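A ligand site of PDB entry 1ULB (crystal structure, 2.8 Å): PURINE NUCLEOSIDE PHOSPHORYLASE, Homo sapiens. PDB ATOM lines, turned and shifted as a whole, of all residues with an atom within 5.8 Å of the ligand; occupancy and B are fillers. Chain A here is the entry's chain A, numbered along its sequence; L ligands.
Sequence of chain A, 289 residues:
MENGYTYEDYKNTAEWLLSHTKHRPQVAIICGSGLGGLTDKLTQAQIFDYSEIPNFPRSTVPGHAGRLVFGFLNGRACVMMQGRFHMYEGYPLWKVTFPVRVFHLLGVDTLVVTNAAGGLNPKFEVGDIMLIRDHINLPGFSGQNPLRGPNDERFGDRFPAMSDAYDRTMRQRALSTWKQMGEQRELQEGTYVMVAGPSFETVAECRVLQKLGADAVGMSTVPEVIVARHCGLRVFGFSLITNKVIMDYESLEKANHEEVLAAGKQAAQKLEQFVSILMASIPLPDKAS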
ATOM      1  N   ALA A 116      -1.840 -14.852 -19.170  1.00  0.00           N
ATOM      2  CA  ALA A 116      -1.487 -14.730 -20.604  1.00  0.00           C
ATOM      3  C   ALA A 116      -2.263 -13.551 -21.197  1.00  0.00           C
ATOM      4  O   ALA A 116      -3.487 -13.645 -21.411  1.00  0.00           O
ATOM      5  CB  ALA A 116      -1.846 -16.018 -21.338  1.00  0.00           C
ATOM      6  N   ALA A 117      -1.523 -12.478 -21.449  1.00  0.00           N
ATOM      7  CA  ALA A 117      -2.125 -11.215 -21.914  1.00  0.00           C
ATOM      8  C   ALA A 117      -1.718 -10.793 -23.335  1.00  0.00           C
ATOM      9  O   ALA A 117      -0.766 -11.343 -23.913  1.00  0.00           O
ATOM     10  CB  ALA A 117      -1.731 -10.070 -20.981  1.00  0.00           C
ATOM     11  N   GLY A 118      -2.502  -9.801 -23.740  1.00  0.00           N
ATOM     12  CA  GLY A 118      -2.526  -9.152 -25.073  1.00  0.00           C
ATOM     13  C   GLY A 118      -1.163  -8.727 -25.630  1.00  0.00           C
ATOM     14  O   GLY A 118      -0.456  -9.534 -26.248  1.00  0.00           O
ATOM     15  N   VAL A 195     -10.044  -5.923 -19.311  1.00  0.00           N
ATOM     16  CA  VAL A 195     -11.245  -5.858 -20.138  1.00  0.00           C
ATOM     17  C   VAL A 195     -11.991  -7.104 -19.673  1.00  0.00           C
ATOM     18  O   VAL A 195     -11.367  -8.125 -19.414  1.00  0.00           O
ATOM     19  CB  VAL A 195     -10.787  -5.918 -21.591  1.00  0.00           C
ATOM     20  CG1 VAL A 195     -11.868  -6.404 -22.556  1.00  0.00           C
ATOM     21  CG2 VAL A 195     -10.307  -4.568 -22.136  1.00  0.00           C
ATOM     22  N   GLY A 197     -14.944  -8.770 -21.043  1.00  0.00           N
ATOM     23  CA  GLY A 197     -15.600  -9.470 -22.154  1.00  0.00           C
ATOM     24  C   GLY A 197     -14.865 -10.701 -22.694  1.00  0.00           C
ATOM     25  O   GLY A 197     -13.627 -10.690 -22.822  1.00  0.00           O
ATOM     26  N   SER A 199     -15.422 -11.963 -25.809  1.00  0.00           N
ATOM     27  CA  SER A 199     -15.016 -11.691 -27.207  1.00  0.00           C
ATOM     28  C   SER A 199     -13.749 -10.849 -27.157  1.00  0.00           C
ATOM     29  O   SER A 199     -13.408 -10.288 -26.101  1.00  0.00           O
ATOM     30  CB  SER A 199     -16.140 -10.991 -27.959  1.00  0.00           C
ATOM     31  OG  SER A 199     -16.377  -9.722 -27.385  1.00  0.00           O
ATOM     32  N   PHE A 200     -13.063 -10.778 -28.293  1.00  0.00           N
ATOM     33  CA  PHE A 200     -11.776 -10.051 -28.393  1.00  0.00           C
ATOM     34  C   PHE A 200     -12.002  -8.582 -28.868  1.00  0.00           C
ATOM     35  O   PHE A 200     -13.135  -8.162 -29.129  1.00  0.00           O
ATOM     36  CB  PHE A 200     -10.807 -10.855 -29.267  1.00  0.00           C
ATOM     37  CG  PHE A 200     -10.027 -11.966 -28.508  1.00  0.00           C
ATOM     38  CD1 PHE A 200     -10.704 -12.899 -27.693  1.00  0.00           C
ATOM     39  CD2 PHE A 200      -8.631 -12.066 -28.638  1.00  0.00           C
ATOM     40  CE1 PHE A 200      -9.987 -13.910 -27.029  1.00  0.00           C
ATOM     41  CE2 PHE A 200      -7.926 -13.074 -27.965  1.00  0.00           C
ATOM     42  CZ  PHE A 200      -8.601 -14.000 -27.163  1.00  0.00           C
ATOM     43  N   GLU A 201     -10.869  -7.867 -28.968  1.00  0.00           N
ATOM     44  CA  GLU A 201     -10.839  -6.380 -29.144  1.00  0.00           C
ATOM     45  C   GLU A 201     -10.780  -5.818 -30.584  1.00  0.00           C
ATOM     46  O   GLU A 201      -9.843  -6.064 -31.360  1.00  0.00           O
ATOM     47  CB  GLU A 201      -9.617  -5.814 -28.426  1.00  0.00           C
ATOM     48  CG  GLU A 201      -9.872  -5.613 -26.925  1.00  0.00           C
ATOM     49  CD  GLU A 201      -9.298  -6.747 -26.053  1.00  0.00           C
ATOM     50  OE1 GLU A 201      -8.376  -7.511 -26.515  1.00  0.00           O
ATOM     51  OE2 GLU A 201      -9.746  -6.917 -24.853  1.00  0.00           O
ATOM     52  N   VAL A 217      -3.423  -5.949 -22.681  1.00  0.00           N
ATOM     53  CA  VAL A 217      -4.837  -6.113 -22.324  1.00  0.00           C
ATOM     54  C   VAL A 217      -5.086  -7.581 -21.885  1.00  0.00           C
ATOM     55  O   VAL A 217      -4.299  -8.478 -22.209  1.00  0.00           O
ATOM     56  CB  VAL A 217      -5.667  -5.701 -23.544  1.00  0.00           C
ATOM     57  CG1 VAL A 217      -5.308  -6.506 -24.803  1.00  0.00           C
ATOM     58  CG2 VAL A 217      -7.158  -5.850 -23.353  1.00  0.00           C
ATOM     59  N   GLY A 218      -6.183  -7.791 -21.156  1.00  0.00           N
ATOM     60  CA  GLY A 218      -6.527  -9.134 -20.647  1.00  0.00           C
ATOM     61  C   GLY A 218      -7.867  -9.106 -19.892  1.00  0.00           C
ATOM     62  O   GLY A 218      -8.453  -8.028 -19.675  1.00  0.00           O
ATOM     63  N   MET A 219      -8.291 -10.304 -19.511  1.00  0.00           N
ATOM     64  CA  MET A 219      -9.580 -10.536 -18.830  1.00  0.00           C
ATOM     65  C   MET A 219      -9.437 -11.181 -17.447  1.00  0.00           C
ATOM     66  O   MET A 219     -10.200 -12.076 -17.076  1.00  0.00           O
ATOM     67  CB  MET A 219     -10.437 -11.477 -19.664  1.00  0.00           C
ATOM     68  CG  MET A 219      -9.870 -11.681 -21.060  1.00  0.00           C
ATOM     69  SD  MET A 219     -11.048 -12.428 -22.163  1.00  0.00           S
ATOM     70  CE  MET A 219     -10.849 -11.735 -23.781  1.00  0.00           C
ATOM     71  N   THR A 242       1.108 -12.445 -25.867  1.00  0.00           N
ATOM     72  CA  THR A 242       0.921 -13.355 -27.006  1.00  0.00           C
ATOM     73  C   THR A 242       0.267 -12.707 -28.273  1.00  0.00           C
ATOM     74  O   THR A 242      -0.219 -13.399 -29.160  1.00  0.00           O
ATOM     75  CB  THR A 242       0.093 -14.621 -26.670  1.00  0.00           C
ATOM     76  OG1 THR A 242      -1.109 -14.639 -27.430  1.00  0.00           O
ATOM     77  CG2 THR A 242      -0.282 -14.774 -25.198  1.00  0.00           C
ATOM     78  N   ASN A 243       0.187 -11.355 -28.505  1.00  0.00           N
ATOM     79  CA  ASN A 243      -0.373 -10.916 -29.872  1.00  0.00           C
ATOM     80  C   ASN A 243      -0.625  -9.381 -30.161  1.00  0.00           C
ATOM     81  O   ASN A 243       0.319  -8.553 -30.098  1.00  0.00           O
ATOM     82  CB  ASN A 243      -1.709 -11.633 -30.196  1.00  0.00           C
ATOM     83  CG  ASN A 243      -2.711 -11.789 -29.022  1.00  0.00           C
ATOM     84  OD1 ASN A 243      -2.536 -12.668 -28.182  1.00  0.00           O
ATOM     85  ND2 ASN A 243      -3.781 -11.020 -28.960  1.00  0.00           N
ATOM     86  N   LYS A 244      -1.906  -9.142 -30.576  1.00  0.00           N
ATOM     87  CA  LYS A 244      -2.657  -7.844 -30.854  1.00  0.00           C
ATOM     88  C   LYS A 244      -2.511  -7.151 -32.234  1.00  0.00           C
ATOM     89  O   LYS A 244      -1.455  -7.183 -32.878  1.00  0.00           O
ATOM     90  CB  LYS A 244      -2.304  -6.707 -29.904  1.00  0.00           C
ATOM     91  CG  LYS A 244      -3.295  -5.547 -30.054  1.00  0.00           C
ATOM     92  CD  LYS A 244      -4.747  -6.003 -29.857  1.00  0.00           C
ATOM     93  CE  LYS A 244      -4.908  -6.847 -28.593  1.00  0.00           C
ATOM     94  NZ  LYS A 244      -6.282  -7.329 -28.406  1.00  0.00           N
ATOM     95  N   ALA A 255      -6.663 -12.991 -34.186  1.00  0.00           N
ATOM     96  CA  ALA A 255      -6.265 -13.346 -32.816  1.00  0.00           C
ATOM     97  C   ALA A 255      -7.307 -14.270 -32.179  1.00  0.00           C
ATOM     98  O   ALA A 255      -8.386 -13.833 -31.768  1.00  0.00           O
ATOM     99  CB  ALA A 255      -6.152 -12.082 -31.965  1.00  0.00           C
ATOM    100  N   ASN A 256      -6.924 -15.530 -32.113  1.00  0.00           N
ATOM    101  CA  ASN A 256      -7.753 -16.581 -31.532  1.00  0.00           C
ATOM    102  C   ASN A 256      -7.288 -16.888 -30.108  1.00  0.00           C
ATOM    103  O   ASN A 256      -6.423 -16.186 -29.563  1.00  0.00           O
ATOM    104  CB  ASN A 256      -7.629 -17.868 -32.349  1.00  0.00           C
ATOM    105  CG  ASN A 256      -8.008 -17.675 -33.822  1.00  0.00           C
ATOM    106  OD1 ASN A 256      -8.902 -18.344 -34.318  1.00  0.00           O
ATOM    107  ND2 ASN A 256      -7.360 -16.786 -34.557  1.00  0.00           N
HETATM  108  N1  LIG L   1      -5.951 -13.001 -23.797  1.00  0.00           N
HETATM  109  C1  LIG L   1      -5.088 -13.378 -24.841  1.00  0.00           C
HETATM  110  N2  LIG L   1      -5.054 -12.486 -25.846  1.00  0.00           N
HETATM  111  C2  LIG L   1      -5.925 -11.479 -25.387  1.00  0.00           C
HETATM  112  C3  LIG L   1      -6.294 -10.300 -26.044  1.00  0.00           C
HETATM  113  O1  LIG L   1      -5.923  -9.929 -27.157  1.00  0.00           O
HETATM  114  N3  LIG L   1      -7.238  -9.569 -25.320  1.00  0.00           N
HETATM  115  C4  LIG L   1      -7.715  -9.963 -24.106  1.00  0.00           C
HETATM  116  N4  LIG L   1      -8.599  -9.165 -23.494  1.00  0.00           N
HETATM  117  N5  LIG L   1      -7.323 -11.061 -23.483  1.00  0.00           N
HETATM  118  C5  LIG L   1      -6.465 -11.785 -24.169  1.00  0.00           C
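Merely in contact with the ligand: Phe 200, Val 217, Gly 218 and Met 219. The nearest printed residue that does not touch the ligand is Gly 118 (4.1 Å).
O1 of the ligand sits at hydrogen-bond distance from ND2 of Asn 243 (3.0 Å). OE1 of Glu 201 is in hydrogen-bond range of N3 of the ligand, at 2.6 Å. The side-chain amino group (NZ) of Lys 244 lies within hydrogen-bond range of an oxygen (O1) of the ligand (2.9 Å). The backbone carbonyl oxygen (O) of Ala 116 sits at hydrogen-bond distance from a nitrogen (N1) of the ligand.
OG1 of Thr 242 is in hydrogen-bond range of OD1 of Asn 243 (2.5 Å). O of Val 217 sits at hydrogen-bond distance from N of Gly 118 (2.7 Å). O of Gly 118 lies within hydrogen-bond range of N of Asn 243 (3.0 Å). OE1 of Glu 201 is in salt-bridge range of NZ of Lys 244 (2.8 Å). The backbone carbonyl oxygen of Gly 218 is in hydrogen-bond range of the backbone NH of Val 195.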
